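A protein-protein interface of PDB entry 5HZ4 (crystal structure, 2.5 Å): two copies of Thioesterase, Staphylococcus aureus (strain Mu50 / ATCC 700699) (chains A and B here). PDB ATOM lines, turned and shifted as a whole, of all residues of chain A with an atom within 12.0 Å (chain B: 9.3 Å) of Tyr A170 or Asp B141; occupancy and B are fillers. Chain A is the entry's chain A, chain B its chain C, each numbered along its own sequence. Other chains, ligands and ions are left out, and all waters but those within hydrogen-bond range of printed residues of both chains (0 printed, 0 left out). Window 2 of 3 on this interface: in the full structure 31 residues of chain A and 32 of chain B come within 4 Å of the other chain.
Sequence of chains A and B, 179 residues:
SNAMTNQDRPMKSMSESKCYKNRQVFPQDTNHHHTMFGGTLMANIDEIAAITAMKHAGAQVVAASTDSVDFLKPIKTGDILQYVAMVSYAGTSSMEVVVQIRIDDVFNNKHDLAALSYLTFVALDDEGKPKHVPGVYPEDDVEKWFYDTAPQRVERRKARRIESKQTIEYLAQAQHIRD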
ATOM      1  N   ARG A 161     -29.009  28.361  11.294  1.00  0.00           N
ATOM      2  CA  ARG A 161     -29.102  29.578  10.510  1.00  0.00           C
ATOM      3  C   ARG A 161     -27.714  30.148  10.209  1.00  0.00           C
ATOM      4  O   ARG A 161     -27.531  30.768   9.159  1.00  0.00           O
ATOM      5  CB  ARG A 161     -29.958  30.672  11.178  1.00  0.00           C
ATOM      6  CG  ARG A 161     -31.488  30.449  11.262  1.00  0.00           C
ATOM      7  CD  ARG A 161     -32.263  31.699  11.733  1.00  0.00           C
ATOM      8  NE  ARG A 161     -32.085  32.885  10.864  1.00  0.00           N
ATOM      9  CZ  ARG A 161     -32.756  33.183   9.737  1.00  0.00           C
ATOM     10  NH1 ARG A 161     -33.693  32.388   9.218  1.00  0.00           N
ATOM     11  NH2 ARG A 161     -32.457  34.309   9.104  1.00  0.00           N
ATOM     12  N   ILE A 162     -26.707  29.815  11.020  1.00  0.00           N
ATOM     13  CA  ILE A 162     -25.364  30.244  10.655  1.00  0.00           C
ATOM     14  C   ILE A 162     -24.806  29.369   9.510  1.00  0.00           C
ATOM     15  O   ILE A 162     -24.044  29.895   8.698  1.00  0.00           O
ATOM     16  CB  ILE A 162     -24.371  30.349  11.873  1.00  0.00           C
ATOM     17  CG1 ILE A 162     -23.745  29.004  12.311  1.00  0.00           C
ATOM     18  CG2 ILE A 162     -24.940  31.218  13.026  1.00  0.00           C
ATOM     19  CD1 ILE A 162     -22.370  28.814  11.711  1.00  0.00           C
ATOM     20  N   GLU A 163     -25.099  28.058   9.448  1.00  0.00           N
ATOM     21  CA  GLU A 163     -24.618  27.289   8.287  1.00  0.00           C
ATOM     22  C   GLU A 163     -25.405  27.782   7.056  1.00  0.00           C
ATOM     23  O   GLU A 163     -24.930  27.697   5.927  1.00  0.00           O
ATOM     24  CB  GLU A 163     -24.772  25.777   8.473  1.00  0.00           C
ATOM     25  CG  GLU A 163     -23.564  25.052   9.157  1.00  0.00           C
ATOM     26  CD  GLU A 163     -22.415  24.665   8.206  1.00  0.00           C
ATOM     27  OE1 GLU A 163     -22.678  24.206   7.068  1.00  0.00           O
ATOM     28  OE2 GLU A 163     -21.238  24.853   8.599  1.00  0.00           O
ATOM     29  N   SER A 164     -26.621  28.271   7.280  1.00  0.00           N
ATOM     30  CA  SER A 164     -27.364  28.980   6.250  1.00  0.00           C
ATOM     31  C   SER A 164     -26.690  30.308   5.943  1.00  0.00           C
ATOM     32  O   SER A 164     -26.857  30.818   4.831  1.00  0.00           O
ATOM     33  CB  SER A 164     -28.846  29.173   6.618  1.00  0.00           C
ATOM     34  OG  SER A 164     -29.632  28.040   6.245  1.00  0.00           O
ATOM     35  N   LYS A 165     -25.964  30.894   6.908  1.00  0.00           N
ATOM     36  CA  LYS A 165     -25.209  32.126   6.609  1.00  0.00           C
ATOM     37  C   LYS A 165     -24.082  31.835   5.672  1.00  0.00           C
ATOM     38  O   LYS A 165     -23.917  32.540   4.703  1.00  0.00           O
ATOM     39  CB  LYS A 165     -24.605  32.809   7.839  1.00  0.00           C
ATOM     40  CG  LYS A 165     -25.561  33.208   8.947  1.00  0.00           C
ATOM     41  CD  LYS A 165     -26.992  33.393   8.411  1.00  0.00           C
ATOM     42  CE  LYS A 165     -27.985  33.643   9.566  1.00  0.00           C
ATOM     43  NZ  LYS A 165     -29.339  33.129   9.179  1.00  0.00           N
ATOM     44  N   GLN A 166     -23.366  30.744   5.896  1.00  0.00           N
ATOM     45  CA  GLN A 166     -22.311  30.386   4.966  1.00  0.00           C
ATOM     46  C   GLN A 166     -22.787  30.193   3.540  1.00  0.00           C
ATOM     47  O   GLN A 166     -22.227  30.770   2.599  1.00  0.00           O
ATOM     48  CB  GLN A 166     -21.614  29.104   5.411  1.00  0.00           C
ATOM     49  CG  GLN A 166     -21.108  29.116   6.830  1.00  0.00           C
ATOM     50  CD  GLN A 166     -19.852  28.269   7.003  1.00  0.00           C
ATOM     51  OE1 GLN A 166     -19.922  27.142   7.494  1.00  0.00           O
ATOM     52  NE2 GLN A 166     -18.694  28.825   6.637  1.00  0.00           N
ATOM     53  N   THR A 167     -23.885  29.460   3.412  1.00  0.00           N
ATOM     54  CA  THR A 167     -24.445  29.118   2.120  1.00  0.00           C
ATOM     55  C   THR A 167     -24.818  30.327   1.266  1.00  0.00           C
ATOM     56  O   THR A 167     -24.489  30.367   0.077  1.00  0.00           O
ATOM     57  CB  THR A 167     -25.643  28.203   2.320  1.00  0.00           C
ATOM     58  OG1 THR A 167     -25.178  26.983   2.913  1.00  0.00           O
ATOM     59  CG2 THR A 167     -26.307  27.885   0.990  1.00  0.00           C
ATOM     60  N   ILE A 168     -25.493  31.310   1.852  1.00  0.00           N
ATOM     61  CA  ILE A 168     -25.796  32.513   1.079  1.00  0.00           C
ATOM     62  C   ILE A 168     -24.506  33.215   0.666  1.00  0.00           C
ATOM     63  O   ILE A 168     -24.375  33.633  -0.484  1.00  0.00           O
ATOM     64  CB  ILE A 168     -26.729  33.489   1.843  1.00  0.00           C
ATOM     65  CG1 ILE A 168     -26.972  34.741   0.999  1.00  0.00           C
ATOM     66  CG2 ILE A 168     -26.163  33.875   3.204  1.00  0.00           C
ATOM     67  CD1 ILE A 168     -28.215  35.488   1.405  1.00  0.00           C
ATOM     68  N   GLU A 169     -23.556  33.338   1.599  1.00  0.00           N
ATOM     69  CA  GLU A 169     -22.250  33.951   1.307  1.00  0.00           C
ATOM     70  C   GLU A 169     -21.527  33.223   0.186  1.00  0.00           C
ATOM     71  O   GLU A 169     -20.906  33.851  -0.677  1.00  0.00           O
ATOM     72  CB  GLU A 169     -21.371  34.036   2.556  1.00  0.00           C
ATOM     73  CG  GLU A 169     -21.686  35.304   3.354  1.00  0.00           C
ATOM     74  CD  GLU A 169     -21.518  35.130   4.853  1.00  0.00           C
ATOM     75  OE1 GLU A 169     -20.598  34.387   5.273  1.00  0.00           O
ATOM     76  OE2 GLU A 169     -22.342  35.702   5.608  1.00  0.00           O
ATOM     77  N   TYR A 170     -21.573  31.896   0.225  1.00  0.00           N
ATOM     78  CA  TYR A 170     -20.903  31.114  -0.786  1.00  0.00           C
ATOM     79  C   TYR A 170     -21.469  31.414  -2.181  1.00  0.00           C
ATOM     80  O   TYR A 170     -20.719  31.648  -3.128  1.00  0.00           O
ATOM     81  CB  TYR A 170     -21.029  29.628  -0.487  1.00  0.00           C
ATOM     82  CG  TYR A 170     -20.296  28.830  -1.518  1.00  0.00           C
ATOM     83  CD1 TYR A 170     -18.939  28.594  -1.394  1.00  0.00           C
ATOM     84  CD2 TYR A 170     -20.947  28.367  -2.656  1.00  0.00           C
ATOM     85  CE1 TYR A 170     -18.251  27.888  -2.357  1.00  0.00           C
ATOM     86  CE2 TYR A 170     -20.272  27.670  -3.627  1.00  0.00           C
ATOM     87  CZ  TYR A 170     -18.918  27.428  -3.472  1.00  0.00           C
ATOM     88  OH  TYR A 170     -18.214  26.720  -4.427  1.00  0.00           O
ATOM     89  N   LEU A 171     -22.790  31.415  -2.302  1.00  0.00           N
ATOM     90  CA  LEU A 171     -23.440  31.680  -3.584  1.00  0.00           C
ATOM     91  C   LEU A 171     -23.244  33.120  -4.044  1.00  0.00           C
ATOM     92  O   LEU A 171     -22.709  33.358  -5.127  1.00  0.00           O
ATOM     93  CB  LEU A 171     -24.932  31.341  -3.484  1.00  0.00           C
ATOM     94  CG  LEU A 171     -25.198  29.902  -3.017  1.00  0.00           C
ATOM     95  CD1 LEU A 171     -26.673  29.605  -2.839  1.00  0.00           C
ATOM     96  CD2 LEU A 171     -24.575  28.916  -4.000  1.00  0.00           C
ATOM     97  N   MET B  14     -27.217  15.664 -10.055  1.00  0.00           N
ATOM     98  CA  MET B  14     -28.188  16.528  -9.398  1.00  0.00           C
ATOM     99  C   MET B  14     -29.015  17.284 -10.462  1.00  0.00           C
ATOM    100  O   MET B  14     -30.193  17.560 -10.246  1.00  0.00           O
ATOM    101  CB  MET B  14     -27.470  17.474  -8.428  1.00  0.00           C
ATOM    102  CG  MET B  14     -26.845  16.745  -7.231  1.00  0.00           C
ATOM    103  SD  MET B  14     -25.930  17.791  -6.062  1.00  0.00           S
ATOM    104  CE  MET B  14     -27.195  18.918  -5.492  1.00  0.00           C
ATOM    105  N   MET B  86     -33.349  20.544  -6.301  1.00  0.00           N
ATOM    106  CA  MET B  86     -32.407  19.460  -6.627  1.00  0.00           C
ATOM    107  C   MET B  86     -32.370  18.406  -5.525  1.00  0.00           C
ATOM    108  O   MET B  86     -32.473  18.748  -4.345  1.00  0.00           O
ATOM    109  CB  MET B  86     -30.987  19.981  -6.785  1.00  0.00           C
ATOM    110  CG  MET B  86     -30.732  20.836  -7.990  1.00  0.00           C
ATOM    111  SD  MET B  86     -29.039  21.474  -7.924  1.00  0.00           S
ATOM    112  CE  MET B  86     -29.029  22.537  -6.492  1.00  0.00           C
ATOM    113  N   GLN B 100     -34.072  26.200  -3.671  1.00  0.00           N
ATOM    114  CA  GLN B 100     -33.639  27.582  -3.601  1.00  0.00           C
ATOM    115  C   GLN B 100     -34.736  28.441  -4.174  1.00  0.00           C
ATOM    116  O   GLN B 100     -35.270  28.136  -5.252  1.00  0.00           O
ATOM    117  CB  GLN B 100     -32.351  27.808  -4.380  1.00  0.00           C
ATOM    118  CG  GLN B 100     -31.163  27.004  -3.942  1.00  0.00           C
ATOM    119  CD  GLN B 100     -30.109  26.971  -5.060  1.00  0.00           C
ATOM    120  OE1 GLN B 100     -29.576  27.999  -5.462  1.00  0.00           O
ATOM    121  NE2 GLN B 100     -29.865  25.790  -5.603  1.00  0.00           N
ATOM    122  N   LEU B 113     -30.998  35.527  -3.215  1.00  0.00           N
ATOM    123  CA  LEU B 113     -31.516  34.349  -2.532  1.00  0.00           C
ATOM    124  C   LEU B 113     -32.409  34.773  -1.383  1.00  0.00           C
ATOM    125  O   LEU B 113     -31.925  35.261  -0.374  1.00  0.00           O
ATOM    126  CB  LEU B 113     -30.369  33.469  -2.023  1.00  0.00           C
ATOM    127  CG  LEU B 113     -30.764  32.137  -1.361  1.00  0.00           C
ATOM    128  CD1 LEU B 113     -31.595  31.243  -2.276  1.00  0.00           C
ATOM    129  CD2 LEU B 113     -29.530  31.377  -0.835  1.00  0.00           C
ATOM    130  N   PRO B 138     -22.880  15.467  -7.799  1.00  0.00           N
ATOM    131  CA  PRO B 138     -22.818  16.874  -8.190  1.00  0.00           C
ATOM    132  C   PRO B 138     -21.947  17.035  -9.429  1.00  0.00           C
ATOM    133  O   PRO B 138     -21.138  16.148  -9.668  1.00  0.00           O
ATOM    134  CB  PRO B 138     -22.164  17.538  -6.981  1.00  0.00           C
ATOM    135  CG  PRO B 138     -21.267  16.457  -6.439  1.00  0.00           C
ATOM    136  CD  PRO B 138     -21.914  15.141  -6.733  1.00  0.00           C
ATOM    137  N   GLU B 139     -22.118  18.117 -10.190  1.00  0.00           N
ATOM    138  CA  GLU B 139     -21.291  18.382 -11.366  1.00  0.00           C
ATOM    139  C   GLU B 139     -20.655  19.772 -11.323  1.00  0.00           C
ATOM    140  O   GLU B 139     -19.584  19.990 -11.887  1.00  0.00           O
ATOM    141  CB  GLU B 139     -22.110  18.216 -12.644  1.00  0.00           C
ATOM    142  CG  GLU B 139     -22.272  16.755 -13.006  1.00  0.00           C
ATOM    143  CD  GLU B 139     -23.234  16.531 -14.147  1.00  0.00           C
ATOM    144  OE1 GLU B 139     -24.079  17.420 -14.417  1.00  0.00           O
ATOM    145  OE2 GLU B 139     -23.160  15.443 -14.751  1.00  0.00           O
ATOM    146  N   ASP B 140     -21.292  20.709 -10.635  1.00  0.00           N
ATOM    147  CA  ASP B 140     -20.686  22.020 -10.461  1.00  0.00           C
ATOM    148  C   ASP B 140     -20.496  22.266  -8.971  1.00  0.00           C
ATOM    149  O   ASP B 140     -20.901  21.458  -8.132  1.00  0.00           O
ATOM    150  CB  ASP B 140     -21.537  23.133 -11.124  1.00  0.00           C
ATOM    151  CG  ASP B 140     -22.931  23.301 -10.481  1.00  0.00           C
ATOM    152  OD1 ASP B 140     -23.052  23.319  -9.230  1.00  0.00           O
ATOM    153  OD2 ASP B 140     -23.929  23.402 -11.240  1.00  0.00           O
ATOM    154  N   ASP B 141     -19.877  23.388  -8.640  1.00  0.00           N
ATOM    155  CA  ASP B 141     -19.453  23.591  -7.276  1.00  0.00           C
ATOM    156  C   ASP B 141     -20.609  23.988  -6.360  1.00  0.00           C
ATOM    157  O   ASP B 141     -20.550  23.741  -5.159  1.00  0.00           O
ATOM    158  CB  ASP B 141     -18.289  24.593  -7.219  1.00  0.00           C
ATOM    159  CG  ASP B 141     -16.937  23.936  -7.583  1.00  0.00           C
ATOM    160  OD1 ASP B 141     -16.565  22.928  -6.937  1.00  0.00           O
ATOM    161  OD2 ASP B 141     -16.242  24.421  -8.503  1.00  0.00           O
ATOM    162  N   VAL B 142     -21.646  24.615  -6.906  1.00  0.00           N
ATOM    163  CA  VAL B 142     -22.854  24.845  -6.125  1.00  0.00           C
ATOM    164  C   VAL B 142     -23.522  23.502  -5.786  1.00  0.00           C
ATOM    165  O   VAL B 142     -23.895  23.251  -4.628  1.00  0.00           O
ATOM    166  CB  VAL B 142     -23.850  25.730  -6.861  1.00  0.00           C
ATOM    167  CG1 VAL B 142     -25.166  25.777  -6.083  1.00  0.00           C
ATOM    168  CG2 VAL B 142     -23.278  27.133  -7.025  1.00  0.00           C
ATOM    169  N   GLU B 143     -23.654  22.641  -6.794  1.00  0.00           N
ATOM    170  CA  GLU B 143     -24.217  21.320  -6.584  1.00  0.00           C
ATOM    171  C   GLU B 143     -23.355  20.557  -5.571  1.00  0.00           C
ATOM    172  O   GLU B 143     -23.876  19.840  -4.713  1.00  0.00           O
ATOM    173  CB  GLU B 143     -24.362  20.575  -7.917  1.00  0.00           C
ATOM    174  CG  GLU B 143     -25.289  21.328  -8.880  1.00  0.00           C
ATOM    175  CD  GLU B 143     -25.400  20.720 -10.275  1.00  0.00           C
ATOM    176  OE1 GLU B 143     -24.750  19.694 -10.564  1.00  0.00           O
ATOM    177  OE2 GLU B 143     -26.118  21.310 -11.110  1.00  0.00           O
ATOM    178  N   LYS B 144     -22.041  20.736  -5.643  1.00  0.00           N
ATOM    179  CA  LYS B 144     -21.149  20.055  -4.710  1.00  0.00           C
ATOM    180  C   LYS B 144     -21.257  20.597  -3.289  1.00  0.00           C
ATOM    181  O   LYS B 144     -21.122  19.851  -2.319  1.00  0.00           O
ATOM    182  CB  LYS B 144     -19.696  20.170  -5.180  1.00  0.00           C
ATOM    183  CG  LYS B 144     -18.751  19.239  -4.432  1.00  0.00           C
ATOM    184  CD  LYS B 144     -17.352  19.225  -5.022  1.00  0.00           C
ATOM    185  CE  LYS B 144     -16.575  18.005  -4.529  1.00  0.00           C
ATOM    186  NZ  LYS B 144     -16.617  17.843  -3.039  1.00  0.00           N
ATOM    187  N   TRP B 145     -21.535  21.890  -3.169  1.00  0.00           N
ATOM    188  CA  TRP B 145     -21.713  22.498  -1.863  1.00  0.00           C
ATOM    189  C   TRP B 145     -22.875  21.884  -1.095  1.00  0.00           C
ATOM    190  O   TRP B 145     -22.754  21.552   0.089  1.00  0.00           O
ATOM    191  CB  TRP B 145     -21.973  23.988  -1.999  1.00  0.00           C
ATOM    192  CG  TRP B 145     -22.363  24.577  -0.689  1.00  0.00           C
ATOM    193  CD1 TRP B 145     -23.635  24.715  -0.190  1.00  0.00           C
ATOM    194  CD2 TRP B 145     -21.487  25.128   0.296  1.00  0.00           C
ATOM    195  NE1 TRP B 145     -23.597  25.302   1.048  1.00  0.00           N
ATOM    196  CE2 TRP B 145     -22.286  25.570   1.372  1.00  0.00           C
ATOM    197  CE3 TRP B 145     -20.096  25.291   0.377  1.00  0.00           C
ATOM    198  CZ2 TRP B 145     -21.750  26.162   2.510  1.00  0.00           C
ATOM    199  CZ3 TRP B 145     -19.561  25.884   1.507  1.00  0.00           C
ATOM    200  CH2 TRP B 145     -20.386  26.305   2.562  1.00  0.00           C
ATOM    201  N   PHE B 146     -23.999  21.714  -1.779  1.00  0.00           N
ATOM    202  CA  PHE B 146     -25.159  21.159  -1.108  1.00  0.00           C
ATOM    203  C   PHE B 146     -24.935  19.695  -0.833  1.00  0.00           C
ATOM    204  O   PHE B 146     -25.327  19.197   0.217  1.00  0.00           O
ATOM    205  CB  PHE B 146     -26.427  21.363  -1.938  1.00  0.00           C
ATOM    206  CG  PHE B 146     -26.894  22.783  -1.969  1.00  0.00           C
ATOM    207  CD1 PHE B 146     -27.323  23.403  -0.809  1.00  0.00           C
ATOM    208  CD2 PHE B 146     -26.918  23.496  -3.150  1.00  0.00           C
ATOM    209  CE1 PHE B 146     -27.766  24.695  -0.832  1.00  0.00           C
ATOM    210  CE2 PHE B 146     -27.357  24.798  -3.170  1.00  0.00           C
ATOM    211  CZ  PHE B 146     -27.784  25.395  -2.012  1.00  0.00           C
ATOM    212  N   TYR B 147     -24.266  19.032  -1.768  1.00  0.00           N
ATOM    213  CA  TYR B 147     -23.954  17.612  -1.663  1.00  0.00           C
ATOM    214  C   TYR B 147     -23.038  17.364  -0.483  1.00  0.00           C
ATOM    215  O   TYR B 147     -23.267  16.445   0.302  1.00  0.00           O
ATOM    216  CB  TYR B 147     -23.295  17.110  -2.961  1.00  0.00           C
ATOM    217  CG  TYR B 147     -22.943  15.637  -2.966  1.00  0.00           C
ATOM    218  CD1 TYR B 147     -21.658  15.214  -2.661  1.00  0.00           C
ATOM    219  CD2 TYR B 147     -23.901  14.664  -3.243  1.00  0.00           C
ATOM    220  CE1 TYR B 147     -21.328  13.874  -2.650  1.00  0.00           C
ATOM    221  CE2 TYR B 147     -23.574  13.313  -3.249  1.00  0.00           C
ATOM    222  CZ  TYR B 147     -22.281  12.931  -2.947  1.00  0.00           C
ATOM    223  OH  TYR B 147     -21.929  11.603  -2.930  1.00  0.00           O
ATOM    224  N   ASP B 148     -22.006  18.195  -0.357  1.00  0.00           N
ATOM    225  CA  ASP B 148     -20.993  18.018   0.687  1.00  0.00           C
ATOM    226  C   ASP B 148     -21.538  18.289   2.070  1.00  0.00           C
ATOM    227  O   ASP B 148     -21.197  17.592   3.023  1.00  0.00           O
ATOM    228  CB  ASP B 148     -19.798  18.949   0.448  1.00  0.00           C
ATOM    229  CG  ASP B 148     -18.886  18.477  -0.664  1.00  0.00           C
ATOM    230  OD1 ASP B 148     -18.904  17.274  -1.018  1.00  0.00           O
ATOM    231  OD2 ASP B 148     -18.161  19.332  -1.215  1.00  0.00           O
ATOM    232  N   THR B 149     -22.429  19.267   2.168  1.00  0.00           N
ATOM    233  CA  THR B 149     -22.967  19.654   3.461  1.00  0.00           C
ATOM    234  C   THR B 149     -24.173  18.793   3.805  1.00  0.00           C
ATOM    235  O   THR B 149     -24.634  18.771   4.948  1.00  0.00           O
ATOM    236  CB  THR B 149     -23.377  21.125   3.468  1.00  0.00           C
ATOM    237  OG1 THR B 149     -24.275  21.366   2.380  1.00  0.00           O
ATOM    238  CG2 THR B 149     -22.158  22.031   3.327  1.00  0.00           C
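CE1 of Phe B146 touches CG2 of Thr A167, at 3.95 Å. Tyr A170 touches Asp B141. Tyr A170 touches Trp B145 (CD1 to CE3, 3.9 Å). CD1 of Leu A171 touches CD2 of Leu B113, 3.9 Å away. CD2 of Leu A171 touches CG2 of Val B142, 3.7 Å away.
Of the 11 printed residues of chain A, 3 touch a printed residue of chain B. Hydrophobic or aromatic side chains of chain A that line the printed part of chain B: Tyr A170 and Leu A171. Along chain A the printed residues that touch a printed residue of chain B span positions 167 to 171. Among the printed residues, 6 pairs touch across the chains.
The indole nitrogen (NE1) of Trp B145 lies within hydrogen-bond range of the side-chain hydroxyl (OG1) of Thr A167 (3.0 Å).
Of chain B, only Asp B141 and Trp B145 come within 4 Å of Tyr A170. Of chain A, only Tyr A170 comes within 4 Å of Asp B141. Asp B140 touches none of the printed residues of chain A. Of chain A, only Leu A171 comes within 4 Å of Val B142. No residue of chain A comes within 4 Å of Glu B143. No residue of chain A comes within 4 Å of Lys B144. Trp B145 touches two residues of chain A. Printed residues of chain B within 4 Å of Thr A167: Trp B145 (3.0 Å) and Phe B146 (3.95 Å). Of the printed residues of chain A, Phe B146 touches Thr A167 (3.95 Å). Ser A164 touches none of the printed residues of chain B. The nearest residue of chain B that does not touch Tyr A170 is Val B142 (4.6 Å).
No position is printed for both chains.
O of Phe B146 lies within hydrogen-bond range of OG1 of Thr B149, 3.2 Å away. The backbone NH of Val B142 sits at hydrogen-bond distance from the side-chain carboxylate of Asp B140, 3.0 Å away. The backbone carbonyl oxygen (O) of Glu A163 is in hydrogen-bond range of the side-chain hydroxyl (OG1) of Thr A167 (3.1 Å). The backbone carbonyl oxygen (O) of Trp B145 sits at hydrogen-bond distance from the side-chain hydroxyl (OG1) of Thr B149, 2.8 Å away.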
